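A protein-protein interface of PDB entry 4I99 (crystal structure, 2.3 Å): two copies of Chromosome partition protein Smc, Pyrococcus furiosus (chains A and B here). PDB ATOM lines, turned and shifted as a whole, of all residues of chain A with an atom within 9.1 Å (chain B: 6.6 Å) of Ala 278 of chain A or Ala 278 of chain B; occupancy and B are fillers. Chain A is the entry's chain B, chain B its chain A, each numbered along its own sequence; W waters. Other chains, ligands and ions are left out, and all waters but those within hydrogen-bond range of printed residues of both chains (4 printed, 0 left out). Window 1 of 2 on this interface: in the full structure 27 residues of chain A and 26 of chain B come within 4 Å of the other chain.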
ATOM      1  N   ASN A  35      30.482  -2.012 -11.367  1.00  0.00           N
ATOM      2  CA  ASN A  35      29.930  -1.661 -12.677  1.00  0.00           C
ATOM      3  C   ASN A  35      30.559  -2.606 -13.704  1.00  0.00           C
ATOM      4  O   ASN A  35      31.739  -2.940 -13.591  1.00  0.00           O
ATOM      5  CB  ASN A  35      30.319  -0.231 -13.076  1.00  0.00           C
ATOM      6  CG  ASN A  35      29.606   0.849 -12.270  1.00  0.00           C
ATOM      7  OD1 ASN A  35      30.168   1.926 -12.053  1.00  0.00           O
ATOM      8  ND2 ASN A  35      28.363   0.589 -11.855  1.00  0.00           N
ATOM      9  N   GLN A 145      16.642  -0.790 -16.072  1.00  0.00           N
ATOM     10  CA  GLN A 145      17.280   0.509 -15.911  1.00  0.00           C
ATOM     11  C   GLN A 145      16.643   1.491 -16.882  1.00  0.00           C
ATOM     12  O   GLN A 145      16.493   1.193 -18.062  1.00  0.00           O
ATOM     13  CB  GLN A 145      18.791   0.408 -16.155  1.00  0.00           C
ATOM     14  CG  GLN A 145      19.609   0.611 -14.889  1.00  0.00           C
ATOM     15  CD  GLN A 145      21.100   0.508 -15.126  1.00  0.00           C
ATOM     16  OE1 GLN A 145      21.677   1.290 -15.883  1.00  0.00           O
ATOM     17  NE2 GLN A 145      21.735  -0.465 -14.480  1.00  0.00           N
ATOM     18  N   GLY A 146      16.236   2.647 -16.367  1.00  0.00           N
ATOM     19  CA  GLY A 146      15.611   3.651 -17.206  1.00  0.00           C
ATOM     20  C   GLY A 146      14.102   3.554 -17.330  1.00  0.00           C
ATOM     21  O   GLY A 146      13.471   4.499 -17.797  1.00  0.00           O
ATOM     22  N   ILE A 148      12.016   3.174 -14.803  1.00  0.00           N
ATOM     23  CA  ILE A 148      11.417   3.810 -13.640  1.00  0.00           C
ATOM     24  C   ILE A 148      10.445   4.940 -13.970  1.00  0.00           C
ATOM     25  O   ILE A 148       9.291   4.912 -13.534  1.00  0.00           O
ATOM     26  CB  ILE A 148      12.502   4.325 -12.651  1.00  0.00           C
ATOM     27  CG1 ILE A 148      11.864   4.586 -11.290  1.00  0.00           C
ATOM     28  CG2 ILE A 148      13.173   5.585 -13.193  1.00  0.00           C
ATOM     29  CD1 ILE A 148      11.075   3.403 -10.763  1.00  0.00           C
ATOM     30  N   GLY A 248      15.038  14.150 -10.754  1.00  0.00           N
ATOM     31  CA  GLY A 248      15.213  12.713 -10.865  1.00  0.00           C
ATOM     32  C   GLY A 248      14.707  11.897  -9.689  1.00  0.00           C
ATOM     33  O   GLY A 248      14.015  10.893  -9.875  1.00  0.00           O
ATOM     34  N   GLY A 249      15.051  12.319  -8.477  1.00  0.00           N
ATOM     35  CA  GLY A 249      14.622  11.592  -7.293  1.00  0.00           C
ATOM     36  C   GLY A 249      13.118  11.602  -7.076  1.00  0.00           C
ATOM     37  O   GLY A 249      12.523  10.575  -6.727  1.00  0.00           O
ATOM     38  N   ALA A 252      11.441   9.330  -9.494  1.00  0.00           N
ATOM     39  CA  ALA A 252      11.646   7.957  -9.059  1.00  0.00           C
ATOM     40  C   ALA A 252      10.681   7.605  -7.920  1.00  0.00           C
ATOM     41  O   ALA A 252      10.060   6.553  -7.935  1.00  0.00           O
ATOM     42  CB  ALA A 252      13.093   7.770  -8.600  1.00  0.00           C
ATOM     43  N   LEU A 256       7.815   4.800  -8.080  1.00  0.00           N
ATOM     44  CA  LEU A 256       7.869   3.701  -7.123  1.00  0.00           C
ATOM     45  C   LEU A 256       6.593   3.611  -6.274  1.00  0.00           C
ATOM     46  O   LEU A 256       6.057   2.523  -6.069  1.00  0.00           O
ATOM     47  CB  LEU A 256       9.109   3.846  -6.229  1.00  0.00           C
ATOM     48  CG  LEU A 256      10.433   3.554  -6.951  1.00  0.00           C
ATOM     49  CD1 LEU A 256      11.616   3.960  -6.093  1.00  0.00           C
ATOM     50  CD2 LEU A 256      10.508   2.080  -7.286  1.00  0.00           C
ATOM     51  N   ASP A 274      16.044  -2.717 -11.487  1.00  0.00           N
ATOM     52  CA  ASP A 274      17.446  -2.522 -11.856  1.00  0.00           C
ATOM     53  C   ASP A 274      17.893  -1.091 -11.536  1.00  0.00           C
ATOM     54  O   ASP A 274      17.705  -0.177 -12.339  1.00  0.00           O
ATOM     55  CB  ASP A 274      17.669  -2.784 -13.348  1.00  0.00           C
ATOM     56  CG  ASP A 274      19.157  -2.831 -13.718  1.00  0.00           C
ATOM     57  OD1 ASP A 274      19.969  -2.191 -13.016  1.00  0.00           O
ATOM     58  OD2 ASP A 274      19.523  -3.496 -14.715  1.00  0.00           O
ATOM     59  N   GLU A 275      18.480  -0.900 -10.360  1.00  0.00           N
ATOM     60  CA  GLU A 275      18.967   0.412  -9.949  1.00  0.00           C
ATOM     61  C   GLU A 275      17.898   1.505  -9.927  1.00  0.00           C
ATOM     62  O   GLU A 275      18.092   2.601 -10.468  1.00  0.00           O
ATOM     63  CB  GLU A 275      20.137   0.831 -10.851  1.00  0.00           C
ATOM     64  CG  GLU A 275      21.422   0.070 -10.546  1.00  0.00           C
ATOM     65  CD  GLU A 275      22.603   0.530 -11.380  1.00  0.00           C
ATOM     66  OE1 GLU A 275      22.763   1.760 -11.555  1.00  0.00           O
ATOM     67  OE2 GLU A 275      23.380  -0.340 -11.848  1.00  0.00           O
ATOM     68  N   ILE A 276      16.763   1.200  -9.309  1.00  0.00           N
ATOM     69  CA  ILE A 276      15.689   2.176  -9.218  1.00  0.00           C
ATOM     70  C   ILE A 276      16.056   3.225  -8.174  1.00  0.00           C
ATOM     71  O   ILE A 276      15.386   4.256  -8.042  1.00  0.00           O
ATOM     72  CB  ILE A 276      14.325   1.488  -8.870  1.00  0.00           C
ATOM     73  CG1 ILE A 276      14.471   0.513  -7.696  1.00  0.00           C
ATOM     74  CG2 ILE A 276      13.826   0.710 -10.083  1.00  0.00           C
ATOM     75  CD1 ILE A 276      14.639   1.148  -6.335  1.00  0.00           C
ATOM     76  N   ASP A 277      17.140   2.965  -7.448  1.00  0.00           N
ATOM     77  CA  ASP A 277      17.611   3.876  -6.415  1.00  0.00           C
ATOM     78  C   ASP A 277      18.750   4.780  -6.869  1.00  0.00           C
ATOM     79  O   ASP A 277      19.350   5.485  -6.064  1.00  0.00           O
ATOM     80  CB  ASP A 277      18.020   3.091  -5.158  1.00  0.00           C
ATOM     81  CG  ASP A 277      18.972   1.920  -5.452  1.00  0.00           C
ATOM     82  OD1 ASP A 277      19.227   1.595  -6.630  1.00  0.00           O
ATOM     83  OD2 ASP A 277      19.464   1.307  -4.476  1.00  0.00           O
ATOM     84  N   ALA A 278      19.035   4.780  -8.165  1.00  0.00           N
ATOM     85  CA  ALA A 278      20.110   5.610  -8.704  1.00  0.00           C
ATOM     86  C   ALA A 278      19.981   7.090  -8.319  1.00  0.00           C
ATOM     87  O   ALA A 278      20.964   7.722  -7.933  1.00  0.00           O
ATOM     88  CB  ALA A 278      20.155   5.466 -10.218  1.00  0.00           C
ATOM     89  N   HIS A 279      18.766   7.634  -8.407  1.00  0.00           N
ATOM     90  CA  HIS A 279      18.525   9.044  -8.088  1.00  0.00           C
ATOM     91  C   HIS A 279      17.903   9.341  -6.723  1.00  0.00           C
ATOM     92  O   HIS A 279      17.452  10.460  -6.497  1.00  0.00           O
ATOM     93  CB  HIS A 279      17.649   9.686  -9.177  1.00  0.00           C
ATOM     94  CG  HIS A 279      18.321   9.783 -10.509  1.00  0.00           C
ATOM     95  ND1 HIS A 279      19.370  10.645 -10.752  1.00  0.00           N
ATOM     96  CD2 HIS A 279      18.149   9.068 -11.648  1.00  0.00           C
ATOM     97  CE1 HIS A 279      19.821  10.453 -11.982  1.00  0.00           C
ATOM     98  NE2 HIS A 279      19.097   9.502 -12.546  1.00  0.00           N
ATOM     99  N   LEU A 280      17.876   8.363  -5.819  1.00  0.00           N
ATOM    100  CA  LEU A 280      17.302   8.571  -4.491  1.00  0.00           C
ATOM    101  C   LEU A 280      18.391   8.945  -3.503  1.00  0.00           C
ATOM    102  O   LEU A 280      19.529   8.503  -3.656  1.00  0.00           O
ATOM    103  CB  LEU A 280      16.622   7.296  -3.999  1.00  0.00           C
ATOM    104  CG  LEU A 280      15.519   6.679  -4.857  1.00  0.00           C
ATOM    105  CD1 LEU A 280      14.993   5.434  -4.144  1.00  0.00           C
ATOM    106  CD2 LEU A 280      14.387   7.688  -5.092  1.00  0.00           C
ATOM    107  N   ASP A 281      18.074   9.760  -2.499  1.00  0.00           N
ATOM    108  CA  ASP A 281      19.103  10.096  -1.513  1.00  0.00           C
ATOM    109  C   ASP A 281      19.127   8.968  -0.472  1.00  0.00           C
ATOM    110  O   ASP A 281      18.203   8.149  -0.431  1.00  0.00           O
ATOM    111  CB  ASP A 281      18.845  11.461  -0.842  1.00  0.00           C
ATOM    112  CG  ASP A 281      17.517  11.529  -0.095  1.00  0.00           C
ATOM    113  OD1 ASP A 281      17.197  10.598   0.680  1.00  0.00           O
ATOM    114  OD2 ASP A 281      16.799  12.541  -0.273  1.00  0.00           O
ATOM    115  N   ASP A 282      20.168   8.912   0.357  1.00  0.00           N
ATOM    116  CA  ASP A 282      20.274   7.850   1.359  1.00  0.00           C
ATOM    117  C   ASP A 282      19.024   7.655   2.201  1.00  0.00           C
ATOM    118  O   ASP A 282      18.619   6.521   2.456  1.00  0.00           O
ATOM    119  CB  ASP A 282      21.474   8.087   2.265  1.00  0.00           C
ATOM    120  CG  ASP A 282      22.778   7.966   1.521  1.00  0.00           C
ATOM    121  OD1 ASP A 282      22.939   6.955   0.798  1.00  0.00           O
ATOM    122  OD2 ASP A 282      23.636   8.873   1.653  1.00  0.00           O
ATOM    123  N   VAL A 285      16.592   5.919   0.031  1.00  0.00           N
ATOM    124  CA  VAL A 285      16.990   4.559  -0.293  1.00  0.00           C
ATOM    125  C   VAL A 285      16.484   3.713   0.880  1.00  0.00           C
ATOM    126  O   VAL A 285      15.893   2.651   0.687  1.00  0.00           O
ATOM    127  CB  VAL A 285      18.525   4.424  -0.423  1.00  0.00           C
ATOM    128  CG1 VAL A 285      18.892   2.977  -0.695  1.00  0.00           C
ATOM    129  CG2 VAL A 285      19.035   5.311  -1.568  1.00  0.00           C
ATOM    130  N   VAL A 288      12.725   3.356   0.767  1.00  0.00           N
ATOM    131  CA  VAL A 288      12.342   2.401  -0.273  1.00  0.00           C
ATOM    132  C   VAL A 288      12.743   0.972   0.135  1.00  0.00           C
ATOM    133  O   VAL A 288      11.998   0.027  -0.095  1.00  0.00           O
ATOM    134  CB  VAL A 288      12.969   2.778  -1.643  1.00  0.00           C
ATOM    135  CG1 VAL A 288      12.846   1.605  -2.637  1.00  0.00           C
ATOM    136  CG2 VAL A 288      12.244   4.003  -2.212  1.00  0.00           C
ATOM    137  N   VAL A 303      16.330  -7.140  -6.527  1.00  0.00           N
ATOM    138  CA  VAL A 303      16.823  -5.779  -6.730  1.00  0.00           C
ATOM    139  C   VAL A 303      18.317  -5.555  -6.986  1.00  0.00           C
ATOM    140  O   VAL A 303      19.152  -5.813  -6.131  1.00  0.00           O
ATOM    141  CB  VAL A 303      16.415  -4.895  -5.512  1.00  0.00           C
ATOM    142  CG1 VAL A 303      16.930  -3.460  -5.684  1.00  0.00           C
ATOM    143  CG2 VAL A 303      14.892  -4.916  -5.334  1.00  0.00           C
ATOM    144  N   ILE A 304      18.637  -5.031  -8.163  1.00  0.00           N
ATOM    145  CA  ILE A 304      20.013  -4.720  -8.506  1.00  0.00           C
ATOM    146  C   ILE A 304      20.295  -3.334  -7.937  1.00  0.00           C
ATOM    147  O   ILE A 304      19.533  -2.389  -8.183  1.00  0.00           O
ATOM    148  CB  ILE A 304      20.207  -4.683 -10.023  1.00  0.00           C
ATOM    149  CG1 ILE A 304      19.844  -6.044 -10.619  1.00  0.00           C
ATOM    150  CG2 ILE A 304      21.645  -4.305 -10.359  1.00  0.00           C
ATOM    151  CD1 ILE A 304      19.710  -6.036 -12.126  1.00  0.00           C
ATOM    152  N   THR A 305      21.380  -3.204  -7.173  1.00  0.00           N
ATOM    153  CA  THR A 305      21.710  -1.918  -6.573  1.00  0.00           C
ATOM    154  C   THR A 305      23.204  -1.673  -6.379  1.00  0.00           C
ATOM    155  O   THR A 305      23.992  -2.610  -6.251  1.00  0.00           O
ATOM    156  CB  THR A 305      21.025  -1.759  -5.202  1.00  0.00           C
ATOM    157  OG1 THR A 305      21.335  -0.466  -4.657  1.00  0.00           O
ATOM    158  CG2 THR A 305      21.517  -2.835  -4.238  1.00  0.00           C
ATOM    159  N   LEU A 306      23.576  -0.398  -6.356  1.00  0.00           N
ATOM    160  CA  LEU A 306      24.958   0.007  -6.145  1.00  0.00           C
ATOM    161  C   LEU A 306      25.054   0.697  -4.786  1.00  0.00           C
ATOM    162  O   LEU A 306      26.151   1.025  -4.325  1.00  0.00           O
ATOM    163  CB  LEU A 306      25.393   0.985  -7.226  1.00  0.00           C
ATOM    164  CG  LEU A 306      25.402   0.433  -8.653  1.00  0.00           C
ATOM    165  CD1 LEU A 306      25.706   1.548  -9.645  1.00  0.00           C
ATOM    166  CD2 LEU A 306      26.437  -0.673  -8.750  1.00  0.00           C
ATOM    167  N   ARG A 307      23.898   0.892  -4.149  1.00  0.00           N
ATOM    168  CA  ARG A 307      23.807   1.580  -2.865  1.00  0.00           C
ATOM    169  C   ARG A 307      23.838   0.648  -1.650  1.00  0.00           C
ATOM    170  O   ARG A 307      23.021  -0.277  -1.534  1.00  0.00           O
ATOM    171  CB  ARG A 307      22.537   2.445  -2.847  1.00  0.00           C
ATOM    172  CG  ARG A 307      22.368   3.304  -4.104  1.00  0.00           C
ATOM    173  CD  ARG A 307      23.433   4.405  -4.214  1.00  0.00           C
ATOM    174  NE  ARG A 307      23.159   5.496  -3.278  1.00  0.00           N
ATOM    175  CZ  ARG A 307      22.232   6.438  -3.465  1.00  0.00           C
ATOM    176  NH1 ARG A 307      21.483   6.446  -4.566  1.00  0.00           N
ATOM    177  NH2 ARG A 307      22.032   7.363  -2.533  1.00  0.00           N
ATOM    178  N   MET A 310      20.761  -0.078   0.414  1.00  0.00           N
ATOM    179  CA  MET A 310      19.829  -1.008  -0.211  1.00  0.00           C
ATOM    180  C   MET A 310      20.206  -2.489  -0.017  1.00  0.00           C
ATOM    181  O   MET A 310      19.354  -3.310   0.340  1.00  0.00           O
ATOM    182  CB  MET A 310      19.699  -0.690  -1.702  1.00  0.00           C
ATOM    183  CG  MET A 310      18.674  -1.542  -2.444  1.00  0.00           C
ATOM    184  SD  MET A 310      16.817  -1.323  -1.868  1.00  0.00           S
ATOM    185  CE  MET A 310      16.426   0.350  -2.786  1.00  0.00           C
ATOM    186  N   ASP B 274      25.021  17.187 -13.354  1.00  0.00           N
ATOM    187  CA  ASP B 274      23.872  16.911 -12.515  1.00  0.00           C
ATOM    188  C   ASP B 274      23.718  15.401 -12.330  1.00  0.00           C
ATOM    189  O   ASP B 274      23.208  14.699 -13.211  1.00  0.00           O
ATOM    190  CB  ASP B 274      22.606  17.478 -13.150  1.00  0.00           C
ATOM    191  CG  ASP B 274      21.444  17.531 -12.179  1.00  0.00           C
ATOM    192  OD1 ASP B 274      21.446  16.758 -11.196  1.00  0.00           O
ATOM    193  OD2 ASP B 274      20.521  18.341 -12.402  1.00  0.00           O
ATOM    194  N   GLU B 275      24.196  14.909 -11.191  1.00  0.00           N
ATOM    195  CA  GLU B 275      24.111  13.495 -10.848  1.00  0.00           C
ATOM    196  C   GLU B 275      24.622  12.551 -11.918  1.00  0.00           C
ATOM    197  O   GLU B 275      23.988  11.541 -12.226  1.00  0.00           O
ATOM    198  CB  GLU B 275      22.671  13.139 -10.478  1.00  0.00           C
ATOM    199  CG  GLU B 275      22.232  13.781  -9.162  1.00  0.00           C
ATOM    200  CD  GLU B 275      20.806  13.434  -8.789  1.00  0.00           C
ATOM    201  OE1 GLU B 275      20.401  12.278  -9.033  1.00  0.00           O
ATOM    202  OE2 GLU B 275      20.097  14.307  -8.244  1.00  0.00           O
ATOM    203  N   ILE B 276      25.779  12.883 -12.476  1.00  0.00           N
ATOM    204  CA  ILE B 276      26.394  12.048 -13.499  1.00  0.00           C
ATOM    205  C   ILE B 276      26.973  10.773 -12.873  1.00  0.00           C
ATOM    206  O   ILE B 276      27.527   9.932 -13.568  1.00  0.00           O
ATOM    207  CB  ILE B 276      27.518  12.823 -14.266  1.00  0.00           C
ATOM    208  CG1 ILE B 276      28.470  13.536 -13.294  1.00  0.00           C
ATOM    209  CG2 ILE B 276      26.891  13.854 -15.199  1.00  0.00           C
ATOM    210  CD1 ILE B 276      29.527  12.659 -12.679  1.00  0.00           C
ATOM    211  N   ASP B 277      26.820  10.631 -11.560  1.00  0.00           N
ATOM    212  CA  ASP B 277      27.328   9.470 -10.838  1.00  0.00           C
ATOM    213  C   ASP B 277      26.218   8.564 -10.325  1.00  0.00           C
ATOM    214  O   ASP B 277      26.471   7.640  -9.555  1.00  0.00           O
ATOM    215  CB  ASP B 277      28.206   9.919  -9.661  1.00  0.00           C
ATOM    216  CG  ASP B 277      27.539  10.984  -8.791  1.00  0.00           C
ATOM    217  OD1 ASP B 277      26.443  11.477  -9.149  1.00  0.00           O
ATOM    218  OD2 ASP B 277      28.122  11.332  -7.746  1.00  0.00           O
ATOM    219  N   ALA B 278      24.989   8.832 -10.764  1.00  0.00           N
ATOM    220  CA  ALA B 278      23.819   8.046 -10.361  1.00  0.00           C
ATOM    221  C   ALA B 278      24.031   6.547 -10.567  1.00  0.00           C
ATOM    222  O   ALA B 278      23.614   5.740  -9.747  1.00  0.00           O
ATOM    223  CB  ALA B 278      22.587   8.499 -11.156  1.00  0.00           C
ATOM    224  N   HIS B 279      24.674   6.186 -11.671  1.00  0.00           N
ATOM    225  CA  HIS B 279      24.914   4.783 -11.995  1.00  0.00           C
ATOM    226  C   HIS B 279      26.347   4.306 -11.822  1.00  0.00           C
ATOM    227  O   HIS B 279      26.726   3.295 -12.402  1.00  0.00           O
ATOM    228  CB  HIS B 279      24.465   4.505 -13.431  1.00  0.00           C
ATOM    229  CG  HIS B 279      22.985   4.560 -13.612  1.00  0.00           C
ATOM    230  ND1 HIS B 279      22.137   3.620 -13.063  1.00  0.00           N
ATOM    231  CD2 HIS B 279      22.195   5.463 -14.245  1.00  0.00           C
ATOM    232  CE1 HIS B 279      20.887   3.946 -13.349  1.00  0.00           C
ATOM    233  NE2 HIS B 279      20.895   5.058 -14.064  1.00  0.00           N
ATOM    234  N   LEU B 280      27.144   5.020 -11.031  1.00  0.00           N
ATOM    235  CA  LEU B 280      28.538   4.625 -10.808  1.00  0.00           C
ATOM    236  C   LEU B 280      28.693   3.908  -9.474  1.00  0.00           C
ATOM    237  O   LEU B 280      28.081   4.311  -8.499  1.00  0.00           O
ATOM    238  CB  LEU B 280      29.449   5.862 -10.823  1.00  0.00           C
ATOM    239  CG  LEU B 280      29.482   6.629 -12.141  1.00  0.00           C
ATOM    240  CD1 LEU B 280      30.352   7.873 -12.005  1.00  0.00           C
ATOM    241  CD2 LEU B 280      30.014   5.711 -13.233  1.00  0.00           C
ATOM    242  N   ASP B 281      29.486   2.840  -9.421  1.00  0.00           N
ATOM    243  CA  ASP B 281      29.693   2.156  -8.148  1.00  0.00           C
ATOM    244  C   ASP B 281      30.628   3.072  -7.364  1.00  0.00           C
ATOM    245  O   ASP B 281      31.196   4.013  -7.933  1.00  0.00           O
ATOM    246  CB  ASP B 281      30.315   0.761  -8.333  1.00  0.00           C
ATOM    247  CG  ASP B 281      31.697   0.796  -8.971  1.00  0.00           C
ATOM    248  OD1 ASP B 281      32.552   1.603  -8.545  1.00  0.00           O
ATOM    249  OD2 ASP B 281      31.933  -0.011  -9.896  1.00  0.00           O
ATOM    250  N   LEU B 306      24.536  12.978  -4.947  1.00  0.00           N
ATOM    251  CA  LEU B 306      23.862  12.370  -3.803  1.00  0.00           C
ATOM    252  C   LEU B 306      24.812  11.355  -3.168  1.00  0.00           C
ATOM    253  O   LEU B 306      24.468  10.690  -2.190  1.00  0.00           O
ATOM    254  CB  LEU B 306      22.590  11.658  -4.263  1.00  0.00           C
ATOM    255  CG  LEU B 306      21.518  12.539  -4.903  1.00  0.00           C
ATOM    256  CD1 LEU B 306      20.400  11.674  -5.473  1.00  0.00           C
ATOM    257  CD2 LEU B 306      20.971  13.500  -3.857  1.00  0.00           C
ATOM    258  N   ARG B 307      26.013  11.250  -3.725  1.00  0.00           N
ATOM    259  CA  ARG B 307      27.014  10.307  -3.238  1.00  0.00           C
ATOM    260  C   ARG B 307      28.036  10.856  -2.250  1.00  0.00           C
ATOM    261  O   ARG B 307      28.729  11.833  -2.543  1.00  0.00           O
ATOM    262  CB  ARG B 307      27.781   9.720  -4.418  1.00  0.00           C
ATOM    263  CG  ARG B 307      26.911   9.018  -5.410  1.00  0.00           C
ATOM    264  CD  ARG B 307      26.094   7.935  -4.749  1.00  0.00           C
ATOM    265  NE  ARG B 307      25.708   6.981  -5.768  1.00  0.00           N
ATOM    266  CZ  ARG B 307      26.464   5.964  -6.163  1.00  0.00           C
ATOM    267  NH1 ARG B 307      27.646   5.748  -5.607  1.00  0.00           N
ATOM    268  NH2 ARG B 307      26.053   5.192  -7.156  1.00  0.00           N
HETATM  269  O   HOH W   1      22.216  10.281  -8.382  1.00  0.00           O
HETATM  270  O   HOH W   2      23.229   6.533  -7.070  1.00  0.00           O
HETATM  271  O   HOH W   3      22.463   3.189  -9.409  1.00  0.00           O
HETATM  272  O   HOH W   4      25.515   8.486  -0.649  1.00  0.00           O
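OE1 of Glu 275 of chain B lies within hydrogen-bond range of ND1 of His 279 of chain A, at 2.6 Å.
O of His 279 of chain B sits at hydrogen-bond distance from ND2 of Asn 35 of chain A (3.2 Å).
A ring nitrogen (ND1) of His 279 of chain B lies within hydrogen-bond range of the side-chain carboxylate of Glu 275 of chain A (2.5 Å).
The backbone NH (N) of Asp 281 of chain B is in hydrogen-bond range of the side-chain amide oxygen (OD1) of Asn 35 of chain A (2.9 Å).
O of Asp 277 of chain B sits at hydrogen-bond distance from NH2 of Arg 307 of chain B, 3.5 Å away.
The side-chain amide nitrogen of Gln 145 of chain A is in hydrogen-bond range of the side-chain carboxylate of Asp 274 of chain A, 2.9 Å away.
N of Glu 275 of chain A is in hydrogen-bond range of O of Ile 304 of chain A (2.8 Å).
The backbone carbonyl oxygen of Leu 280 of chain A lies within hydrogen-bond range of the guanidinium group of Arg 307 of chain A (3.0 Å).
OD1 of Asp 282 of chain A is in salt-bridge range of NH2 of Arg 307 of chain A (3.5 Å).
The side-chain hydroxyl (OG1) of Thr 305 of chain A is in hydrogen-bond range of the backbone NH (N) of Arg 307 of chain A.
Asn 35 of chain A touches Leu 280 of chain B.
Gln 145 of chain A touches His 279 of chain B.
Ala 278 of chain A touches Ala 278 of chain B.
Ala 278 of chain A touches His 279 of chain B.
His 279 of chain A touches Ala 278 of chain B.
Leu 306 of chain B touches His 279 of chain A.
Leu 280 of chain A touches Leu 306 of chain B.
Leu 306 of chain A touches His 279 of chain B (CD1 to O, 3.4 Å).
Leu 306 of chain A touches Leu 280 of chain B (CD1 to C, 3.8 Å).
NE of Arg 307 of chain B touches CD of Arg 307 of chain A, at 3.8 Å.
Ala 278 of chain A touches just these residues of chain B: Ala 278 and His 279.
Ala 278 of chain B touches just these residues of chain A: Ala 278 (3.5 Å) and His 279 (3.5 Å).
No residue of chain A comes within 4 Å of Asp 277 of chain B.
His 279 of chain B touches just these residues of chain A: Asn 35 (3.2 Å), Gln 145 (3.7 Å), Glu 275 (2.5 Å), Ala 278 (3.6 Å) and Leu 306 (3.4 Å).
Printed residues of chain B within 4 Å of Leu 280 of chain A: Leu 306 (3.8 Å).
Of the printed residues of chain A, Glu 275 of chain B touches His 279 (2.6 Å).
Asp 282 of chain A touches none of the printed residues of chain B.
Hydrophobic or aromatic side chains of chain B that line the printed part of chain A: Ala 278, His 279, Leu 280 and Leu 306.
Printed residues of chain A that touch a printed residue of chain B: Asn 35, Gln 145, Glu 275, Ala 278, His 279, Leu 280, Leu 306 and Arg 307.
Hydrophobic or aromatic side chains of chain A that line the printed part of chain B: Ala 278, His 279 and Leu 306.
Among the printed residues, 14 pairs touch across the chains.
Glu 275 of chain A touches His 279 of chain B, and with the chains exchanged His 279 of chain A touches Glu 275 of chain B.
His 279 of chain A touches Leu 306 of chain B, and with the chains exchanged Leu 306 of chain A touches His 279 of chain B.
Leu 280 of chain A touches Leu 306 of chain B, and with the chains exchanged Leu 306 of chain A touches Leu 280 of chain B.
Arg 307 of chain B touches its own counterpart, Arg 307 of chain A.
Of the 14 pairs that touch across the chains among the printed residues, 10 have their exchanged pair printed and touching as well.
Water W3 bridges OE1 of Glu 275 of chain A and O of Ala 278 of chain B.
Water W2 lies within hydrogen-bond range of O of Ala 278 of chain A (2.7 Å), O of Ala 278 of chain B (2.8 Å), NE of Arg 307 of chain B (2.8 Å) and NH1 of Arg 307 of chain A (3.1 Å).
Water W1 lies within hydrogen-bond range of OE1 of Glu 275 of chain B (2.8 Å) and O of Ala 278 of chain A (2.9 Å).
Water W4 bridges the backbone carbonyl oxygen (O) of Leu 306 of chain B (2.9 Å) and the side-chain carboxylate (OD2) of Asp 282 of chain A (3.0 Å).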
